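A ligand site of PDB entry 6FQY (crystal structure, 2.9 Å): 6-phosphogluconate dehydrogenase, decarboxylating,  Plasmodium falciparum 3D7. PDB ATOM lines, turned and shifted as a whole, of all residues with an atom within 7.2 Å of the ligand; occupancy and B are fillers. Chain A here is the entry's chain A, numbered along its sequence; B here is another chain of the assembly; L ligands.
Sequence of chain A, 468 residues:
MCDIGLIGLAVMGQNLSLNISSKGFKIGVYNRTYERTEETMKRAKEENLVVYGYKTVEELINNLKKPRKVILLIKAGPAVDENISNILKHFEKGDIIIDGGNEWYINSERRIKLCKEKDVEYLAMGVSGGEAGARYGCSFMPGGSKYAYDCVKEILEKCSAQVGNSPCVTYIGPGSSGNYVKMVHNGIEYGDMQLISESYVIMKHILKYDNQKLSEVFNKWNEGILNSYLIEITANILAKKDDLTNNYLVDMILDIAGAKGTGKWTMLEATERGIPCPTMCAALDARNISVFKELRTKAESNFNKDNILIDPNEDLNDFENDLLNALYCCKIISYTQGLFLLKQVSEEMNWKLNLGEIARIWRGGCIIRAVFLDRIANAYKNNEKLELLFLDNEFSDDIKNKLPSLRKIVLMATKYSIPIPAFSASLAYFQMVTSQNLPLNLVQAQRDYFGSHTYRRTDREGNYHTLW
CA of Gly 8 touches O5 of the ligand (3.9 Å). Ala 10 touches the ligand. CA of Ile 74 touches O4 of the ligand, 3.8 Å away. Ala 79 touches the ligand. Nine residues have an atom within 4 Å of the ligand: Gly 8, Ala 10, Asn 31, Arg 32, Thr 33, Arg 36, Ile 74, Lys 75 and Ala 79. The nearest printed residue that does not touch the ligand is Leu 9 (4.001 Å).
O12 of the ligand lies within hydrogen-bond range of ND2 of Asn 31. The backbone NH of Thr 33 lies close to an oxygen (O13) of the ligand (3.5 Å). The guanidinium group of Arg 32 is in salt-bridge range of an oxygen (O13) of the ligand, at 3.4 Å. O12 of the ligand is in salt-bridge range of NH2 of Arg 36, at 2.9 Å. The backbone NH (N) of Lys 75 sits at hydrogen-bond distance from an oxygen (O4) of the ligand (3.3 Å).
ND2 of Asn 83 is in hydrogen-bond range of O of Ala 79 (2.7 Å). ND2 of Asn 31 lies within hydrogen-bond range of O of Thr 33, 3.1 Å away. The backbone NH (N) of Leu 9 is in hydrogen-bond range of the side-chain amide oxygen (OD1) of Asn 31 (2.7 Å). The backbone carbonyl oxygen (O) of Leu 9 sits at hydrogen-bond distance from the guanidinium group (NE) of Arg 36 (3.2 Å). The backbone carbonyl oxygen (O) of Tyr 30 sits at hydrogen-bond distance from the backbone NH (N) of Gly 8, at 3.3 Å.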
ATOM      1  N   ILE A   7     -25.520 -23.247 -23.788  1.00  0.00           N
ATOM      2  CA  ILE A   7     -24.627 -24.391 -23.969  1.00  0.00           C
ATOM      3  C   ILE A   7     -23.449 -24.222 -23.013  1.00  0.00           C
ATOM      4  O   ILE A   7     -22.884 -23.129 -22.904  1.00  0.00           O
ATOM      5  CB  ILE A   7     -24.152 -24.532 -25.420  1.00  0.00           C
ATOM      6  CG1 ILE A   7     -25.119 -25.372 -26.269  1.00  0.00           C
ATOM      7  CG2 ILE A   7     -22.764 -25.164 -25.487  1.00  0.00           C
ATOM      8  CD1 ILE A   7     -26.521 -24.842 -26.346  1.00  0.00           C
ATOM      9  N   GLY A   8     -23.089 -25.299 -22.310  1.00  0.00           N
ATOM     10  CA  GLY A   8     -21.918 -25.281 -21.457  1.00  0.00           C
ATOM     11  C   GLY A   8     -22.214 -24.923 -20.018  1.00  0.00           C
ATOM     12  O   GLY A   8     -22.308 -23.742 -19.662  1.00  0.00           O
ATOM     13  N   LEU A   9     -22.364 -25.939 -19.174  1.00  0.00           N
ATOM     14  CA  LEU A   9     -22.721 -25.791 -17.770  1.00  0.00           C
ATOM     15  C   LEU A   9     -21.522 -26.059 -16.873  1.00  0.00           C
ATOM     16  O   LEU A   9     -21.390 -27.137 -16.298  1.00  0.00           O
ATOM     17  CB  LEU A   9     -23.858 -26.708 -17.428  1.00  0.00           C
ATOM     18  CG  LEU A   9     -25.252 -26.363 -17.941  1.00  0.00           C
ATOM     19  CD1 LEU A   9     -25.354 -26.545 -19.434  1.00  0.00           C
ATOM     20  CD2 LEU A   9     -26.189 -27.299 -17.249  1.00  0.00           C
ATOM     21  N   ALA A  10     -20.655 -25.070 -16.733  1.00  0.00           N
ATOM     22  CA  ALA A  10     -19.606 -25.174 -15.727  1.00  0.00           C
ATOM     23  C   ALA A  10     -20.118 -24.548 -14.435  1.00  0.00           C
ATOM     24  O   ALA A  10     -21.321 -24.551 -14.170  1.00  0.00           O
ATOM     25  CB  ALA A  10     -18.320 -24.488 -16.193  1.00  0.00           C
ATOM     26  N   VAL A  11     -19.215 -23.989 -13.620  1.00  0.00           N
ATOM     27  CA  VAL A  11     -19.658 -23.239 -12.449  1.00  0.00           C
ATOM     28  C   VAL A  11     -20.183 -21.876 -12.853  1.00  0.00           C
ATOM     29  O   VAL A  11     -20.799 -21.183 -12.035  1.00  0.00           O
ATOM     30  CB  VAL A  11     -18.521 -23.103 -11.420  1.00  0.00           C
ATOM     31  CG1 VAL A  11     -17.508 -22.073 -11.874  1.00  0.00           C
ATOM     32  CG2 VAL A  11     -19.073 -22.778 -10.033  1.00  0.00           C
ATOM     33  N   MET A  12     -19.970 -21.481 -14.112  1.00  0.00           N
ATOM     34  CA  MET A  12     -20.298 -20.157 -14.601  1.00  0.00           C
ATOM     35  C   MET A  12     -21.636 -20.101 -15.325  1.00  0.00           C
ATOM     36  O   MET A  12     -22.411 -19.171 -15.116  1.00  0.00           O
ATOM     37  CB  MET A  12     -19.195 -19.689 -15.560  1.00  0.00           C
ATOM     38  CG  MET A  12     -19.243 -18.232 -15.951  1.00  0.00           C
ATOM     39  SD  MET A  12     -18.795 -17.169 -14.575  1.00  0.00           S
ATOM     40  CE  MET A  12     -17.170 -17.811 -14.176  1.00  0.00           C
ATOM     41  N   TYR A  30     -28.127 -27.540 -22.253  1.00  0.00           N
ATOM     42  CA  TYR A  30     -27.442 -28.693 -22.830  1.00  0.00           C
ATOM     43  C   TYR A  30     -26.012 -28.712 -22.321  1.00  0.00           C
ATOM     44  O   TYR A  30     -25.360 -27.668 -22.264  1.00  0.00           O
ATOM     45  CB  TYR A  30     -27.422 -28.684 -24.373  1.00  0.00           C
ATOM     46  CG  TYR A  30     -26.418 -29.659 -24.982  1.00  0.00           C
ATOM     47  CD1 TYR A  30     -25.076 -29.300 -25.161  1.00  0.00           C
ATOM     48  CD2 TYR A  30     -26.801 -30.943 -25.340  1.00  0.00           C
ATOM     49  CE1 TYR A  30     -24.157 -30.185 -25.689  1.00  0.00           C
ATOM     50  CE2 TYR A  30     -25.879 -31.833 -25.893  1.00  0.00           C
ATOM     51  CZ  TYR A  30     -24.562 -31.449 -26.058  1.00  0.00           C
ATOM     52  OH  TYR A  30     -23.650 -32.330 -26.593  1.00  0.00           O
ATOM     53  N   ASN A  31     -25.519 -29.903 -21.990  1.00  0.00           N
ATOM     54  CA  ASN A  31     -24.101 -30.110 -21.726  1.00  0.00           C
ATOM     55  C   ASN A  31     -23.650 -31.379 -22.441  1.00  0.00           C
ATOM     56  O   ASN A  31     -24.457 -32.293 -22.665  1.00  0.00           O
ATOM     57  CB  ASN A  31     -23.802 -30.215 -20.230  1.00  0.00           C
ATOM     58  CG  ASN A  31     -22.431 -29.663 -19.857  1.00  0.00           C
ATOM     59  OD1 ASN A  31     -22.152 -28.485 -20.069  1.00  0.00           O
ATOM     60  ND2 ASN A  31     -21.588 -30.510 -19.286  1.00  0.00           N
ATOM     61  N   ARG A  32     -22.369 -31.427 -22.799  1.00  0.00           N
ATOM     62  CA  ARG A  32     -21.806 -32.637 -23.396  1.00  0.00           C
ATOM     63  C   ARG A  32     -21.976 -33.829 -22.456  1.00  0.00           C
ATOM     64  O   ARG A  32     -22.356 -34.924 -22.898  1.00  0.00           O
ATOM     65  CB  ARG A  32     -20.348 -32.423 -23.783  1.00  0.00           C
ATOM     66  CG  ARG A  32     -19.670 -33.700 -24.273  1.00  0.00           C
ATOM     67  CD  ARG A  32     -18.213 -33.489 -24.642  1.00  0.00           C
ATOM     68  NE  ARG A  32     -17.305 -33.528 -23.495  1.00  0.00           N
ATOM     69  CZ  ARG A  32     -15.994 -33.404 -23.574  1.00  0.00           C
ATOM     70  NH1 ARG A  32     -15.404 -33.246 -24.749  1.00  0.00           N
ATOM     71  NH2 ARG A  32     -15.246 -33.429 -22.469  1.00  0.00           N
ATOM     72  N   THR A  33     -21.673 -33.649 -21.177  1.00  0.00           N
ATOM     73  CA  THR A  33     -21.913 -34.663 -20.160  1.00  0.00           C
ATOM     74  C   THR A  33     -23.161 -34.271 -19.381  1.00  0.00           C
ATOM     75  O   THR A  33     -23.313 -33.107 -19.003  1.00  0.00           O
ATOM     76  CB  THR A  33     -20.706 -34.808 -19.216  1.00  0.00           C
ATOM     77  OG1 THR A  33     -20.598 -33.635 -18.402  1.00  0.00           O
ATOM     78  CG2 THR A  33     -19.420 -35.009 -19.999  1.00  0.00           C
ATOM     79  N   TYR A  34     -24.035 -35.243 -19.127  1.00  0.00           N
ATOM     80  CA  TYR A  34     -25.370 -34.915 -18.635  1.00  0.00           C
ATOM     81  C   TYR A  34     -25.505 -34.958 -17.120  1.00  0.00           C
ATOM     82  O   TYR A  34     -26.573 -34.613 -16.599  1.00  0.00           O
ATOM     83  CB  TYR A  34     -26.379 -35.895 -19.268  1.00  0.00           C
ATOM     84  CG  TYR A  34     -27.850 -35.619 -18.995  1.00  0.00           C
ATOM     85  CD1 TYR A  34     -28.526 -36.287 -17.983  1.00  0.00           C
ATOM     86  CD2 TYR A  34     -28.560 -34.724 -19.786  1.00  0.00           C
ATOM     87  CE1 TYR A  34     -29.870 -36.033 -17.754  1.00  0.00           C
ATOM     88  CE2 TYR A  34     -29.890 -34.476 -19.563  1.00  0.00           C
ATOM     89  CZ  TYR A  34     -30.545 -35.130 -18.546  1.00  0.00           C
ATOM     90  OH  TYR A  34     -31.881 -34.878 -18.328  1.00  0.00           O
ATOM     91  N   ARG A  36     -23.931 -32.802 -15.213  1.00  0.00           N
ATOM     92  CA  ARG A  36     -24.040 -31.391 -14.855  1.00  0.00           C
ATOM     93  C   ARG A  36     -25.362 -30.784 -15.341  1.00  0.00           C
ATOM     94  O   ARG A  36     -25.880 -29.855 -14.715  1.00  0.00           O
ATOM     95  CB  ARG A  36     -22.845 -30.608 -15.397  1.00  0.00           C
ATOM     96  CG  ARG A  36     -21.545 -30.987 -14.717  1.00  0.00           C
ATOM     97  CD  ARG A  36     -20.598 -29.799 -14.570  1.00  0.00           C
ATOM     98  NE  ARG A  36     -19.634 -29.718 -15.655  1.00  0.00           N
ATOM     99  CZ  ARG A  36     -18.346 -29.404 -15.500  1.00  0.00           C
ATOM    100  NH1 ARG A  36     -17.872 -29.135 -14.286  1.00  0.00           N
ATOM    101  NH2 ARG A  36     -17.542 -29.340 -16.550  1.00  0.00           N
ATOM    102  N   LEU A  73     -20.881 -20.917 -23.080  1.00  0.00           N
ATOM    103  CA  LEU A  73     -19.951 -20.687 -21.981  1.00  0.00           C
ATOM    104  C   LEU A  73     -19.024 -21.875 -21.843  1.00  0.00           C
ATOM    105  O   LEU A  73     -18.796 -22.418 -20.761  1.00  0.00           O
ATOM    106  CB  LEU A  73     -20.696 -20.403 -20.689  1.00  0.00           C
ATOM    107  CG  LEU A  73     -21.468 -19.085 -20.688  1.00  0.00           C
ATOM    108  CD1 LEU A  73     -22.416 -18.989 -19.524  1.00  0.00           C
ATOM    109  CD2 LEU A  73     -20.499 -17.923 -20.672  1.00  0.00           C
ATOM    110  N   ILE A  74     -18.472 -22.305 -22.969  1.00  0.00           N
ATOM    111  CA  ILE A  74     -17.510 -23.412 -23.015  1.00  0.00           C
ATOM    112  C   ILE A  74     -16.112 -22.853 -23.177  1.00  0.00           C
ATOM    113  O   ILE A  74     -15.917 -21.743 -23.699  1.00  0.00           O
ATOM    114  CB  ILE A  74     -17.876 -24.385 -24.148  1.00  0.00           C
ATOM    115  CG1 ILE A  74     -17.617 -23.761 -25.511  1.00  0.00           C
ATOM    116  CG2 ILE A  74     -19.341 -24.796 -24.053  1.00  0.00           C
ATOM    117  CD1 ILE A  74     -17.599 -24.758 -26.610  1.00  0.00           C
ATOM    118  N   LYS A  75     -15.128 -23.614 -22.704  1.00  0.00           N
ATOM    119  CA  LYS A  75     -13.759 -23.140 -22.676  1.00  0.00           C
ATOM    120  C   LYS A  75     -13.185 -23.002 -24.083  1.00  0.00           C
ATOM    121  O   LYS A  75     -13.627 -23.646 -25.036  1.00  0.00           O
ATOM    122  CB  LYS A  75     -12.880 -24.078 -21.840  1.00  0.00           C
ATOM    123  CG  LYS A  75     -12.435 -25.333 -22.571  1.00  0.00           C
ATOM    124  CD  LYS A  75     -11.452 -26.130 -21.734  1.00  0.00           C
ATOM    125  CE  LYS A  75     -10.026 -25.924 -22.207  1.00  0.00           C
ATOM    126  NZ  LYS A  75      -9.078 -26.800 -21.455  1.00  0.00           N
ATOM    127  N   ALA A  76     -12.183 -22.133 -24.205  1.00  0.00           N
ATOM    128  CA  ALA A  76     -11.594 -21.838 -25.512  1.00  0.00           C
ATOM    129  C   ALA A  76     -10.866 -23.068 -26.043  1.00  0.00           C
ATOM    130  O   ALA A  76     -10.065 -23.688 -25.339  1.00  0.00           O
ATOM    131  CB  ALA A  76     -10.644 -20.652 -25.407  1.00  0.00           C
ATOM    132  N   GLY A  77     -11.153 -23.420 -27.297  1.00  0.00           N
ATOM    133  CA  GLY A  77     -10.541 -24.559 -27.932  1.00  0.00           C
ATOM    134  C   GLY A  77     -11.281 -24.937 -29.193  1.00  0.00           C
ATOM    135  O   GLY A  77     -12.177 -24.229 -29.653  1.00  0.00           O
ATOM    136  N   PRO A  78     -10.900 -26.065 -29.807  1.00  0.00           N
ATOM    137  CA  PRO A  78     -11.687 -26.579 -30.944  1.00  0.00           C
ATOM    138  C   PRO A  78     -13.117 -26.893 -30.563  1.00  0.00           C
ATOM    139  O   PRO A  78     -13.980 -26.981 -31.449  1.00  0.00           O
ATOM    140  CB  PRO A  78     -10.918 -27.833 -31.369  1.00  0.00           C
ATOM    141  CG  PRO A  78     -10.149 -28.238 -30.164  1.00  0.00           C
ATOM    142  CD  PRO A  78      -9.787 -26.959 -29.463  1.00  0.00           C
ATOM    143  N   ALA A  79     -13.384 -27.071 -29.267  1.00  0.00           N
ATOM    144  CA  ALA A  79     -14.754 -27.331 -28.814  1.00  0.00           C
ATOM    145  C   ALA A  79     -15.658 -26.165 -29.146  1.00  0.00           C
ATOM    146  O   ALA A  79     -16.861 -26.355 -29.376  1.00  0.00           O
ATOM    147  CB  ALA A  79     -14.758 -27.602 -27.312  1.00  0.00           C
ATOM    148  N   VAL A  80     -15.124 -24.947 -29.164  1.00  0.00           N
ATOM    149  CA  VAL A  80     -15.972 -23.804 -29.476  1.00  0.00           C
ATOM    150  C   VAL A  80     -16.455 -23.908 -30.914  1.00  0.00           C
ATOM    151  O   VAL A  80     -17.618 -23.636 -31.204  1.00  0.00           O
ATOM    152  CB  VAL A  80     -15.223 -22.485 -29.225  1.00  0.00           C
ATOM    153  CG1 VAL A  80     -16.163 -21.298 -29.364  1.00  0.00           C
ATOM    154  CG2 VAL A  80     -14.575 -22.495 -27.858  1.00  0.00           C
ATOM    155  N   GLU A  82     -16.556 -26.816 -32.803  1.00  0.00           N
ATOM    156  CA  GLU A  82     -17.417 -27.970 -32.972  1.00  0.00           C
ATOM    157  C   GLU A  82     -18.821 -27.736 -32.435  1.00  0.00           C
ATOM    158  O   GLU A  82     -19.783 -28.287 -32.974  1.00  0.00           O
ATOM    159  CB  GLU A  82     -16.804 -29.169 -32.227  1.00  0.00           C
ATOM    160  CG  GLU A  82     -17.749 -30.337 -32.054  1.00  0.00           C
ATOM    161  CD  GLU A  82     -17.072 -31.691 -32.092  1.00  0.00           C
ATOM    162  OE1 GLU A  82     -15.855 -31.770 -31.823  1.00  0.00           O
ATOM    163  OE2 GLU A  82     -17.776 -32.687 -32.358  1.00  0.00           O
ATOM    164  N   ASN A  83     -18.970 -26.902 -31.406  1.00  0.00           N
ATOM    165  CA  ASN A  83     -20.314 -26.469 -31.029  1.00  0.00           C
ATOM    166  C   ASN A  83     -20.896 -25.511 -32.057  1.00  0.00           C
ATOM    167  O   ASN A  83     -22.012 -25.724 -32.557  1.00  0.00           O
ATOM    168  CB  ASN A  83     -20.296 -25.840 -29.633  1.00  0.00           C
ATOM    169  CG  ASN A  83     -20.250 -26.888 -28.528  1.00  0.00           C
ATOM    170  OD1 ASN A  83     -21.281 -27.396 -28.090  1.00  0.00           O
ATOM    171  ND2 ASN A  83     -19.047 -27.229 -28.098  1.00  0.00           N
ATOM    172  N   HIS B 453      -9.973 -20.581  -8.102  1.00  0.00           N
ATOM    173  CA  HIS B 453      -8.799 -21.286  -8.587  1.00  0.00           C
ATOM    174  C   HIS B 453      -8.094 -21.955  -7.419  1.00  0.00           C
ATOM    175  O   HIS B 453      -7.874 -21.332  -6.379  1.00  0.00           O
ATOM    176  CB  HIS B 453      -7.852 -20.340  -9.317  1.00  0.00           C
ATOM    177  CG  HIS B 453      -8.463 -19.665 -10.505  1.00  0.00           C
ATOM    178  ND1 HIS B 453      -9.198 -18.501 -10.406  1.00  0.00           N
ATOM    179  CD2 HIS B 453      -8.459 -19.993 -11.822  1.00  0.00           C
ATOM    180  CE1 HIS B 453      -9.609 -18.134 -11.611  1.00  0.00           C
ATOM    181  NE2 HIS B 453      -9.173 -19.024 -12.486  1.00  0.00           N
HETATM  182  P1  LIG L   1     -14.541 -26.672 -17.011  1.00  0.00           P
HETATM  183  O1  LIG L   1     -14.962 -28.000 -16.442  1.00  0.00           O
HETATM  184  O2  LIG L   1     -15.158 -25.558 -16.187  1.00  0.00           O
HETATM  185  O3  LIG L   1     -15.062 -26.550 -18.578  1.00  0.00           O
HETATM  186  C1  LIG L   1     -16.123 -25.676 -18.861  1.00  0.00           C
HETATM  187  C2  LIG L   1     -16.861 -26.145 -20.158  1.00  0.00           C
HETATM  188  O4  LIG L   1     -15.997 -26.366 -21.113  1.00  0.00           O
HETATM  189  C3  LIG L   1     -17.576 -27.480 -19.899  1.00  0.00           C
HETATM  190  O5  LIG L   1     -18.849 -27.433 -20.365  1.00  0.00           O
HETATM  191  C4  LIG L   1     -16.761 -28.510 -20.704  1.00  0.00           C
HETATM  192  O6  LIG L   1     -17.637 -29.635 -21.157  1.00  0.00           O
HETATM  193  C5  LIG L   1     -16.343 -27.820 -21.726  1.00  0.00           C
HETATM  194  N1  LIG L   1     -15.161 -28.418 -22.294  1.00  0.00           N
HETATM  195  C6  LIG L   1     -13.893 -28.422 -21.875  1.00  0.00           C
HETATM  196  N2  LIG L   1     -13.171 -29.133 -22.743  1.00  0.00           N
HETATM  197  C7  LIG L   1     -13.996 -29.566 -23.709  1.00  0.00           C
HETATM  198  C8  LIG L   1     -13.784 -30.324 -24.838  1.00  0.00           C
HETATM  199  N3  LIG L   1     -12.642 -30.962 -25.474  1.00  0.00           N
HETATM  200  N4  LIG L   1     -14.792 -30.620 -25.644  1.00  0.00           N
HETATM  201  C9  LIG L   1     -16.041 -30.184 -25.356  1.00  0.00           C
HETATM  202  N5  LIG L   1     -16.258 -29.428 -24.240  1.00  0.00           N
HETATM  203  C10 LIG L   1     -15.223 -29.124 -23.425  1.00  0.00           C
HETATM  204  O7  LIG L   1     -12.902 -26.547 -16.959  1.00  0.00           O
HETATM  205  P2  LIG L   1     -12.077 -25.149 -17.281  1.00  0.00           P
HETATM  206  O8  LIG L   1     -10.461 -25.412 -17.099  1.00  0.00           O
HETATM  207  O9  LIG L   1     -12.520 -24.065 -16.321  1.00  0.00           O
HETATM  208  O10 LIG L   1     -12.364 -24.708 -18.693  1.00  0.00           O
HETATM  209  P3  LIG L   1     -17.945 -30.862 -20.100  1.00  0.00           P
HETATM  210  O11 LIG L   1     -16.638 -31.383 -19.533  1.00  0.00           O
HETATM  211  O12 LIG L   1     -18.803 -30.350 -18.968  1.00  0.00           O
HETATM  212  O13 LIG L   1     -18.658 -31.967 -20.827  1.00  0.00           O
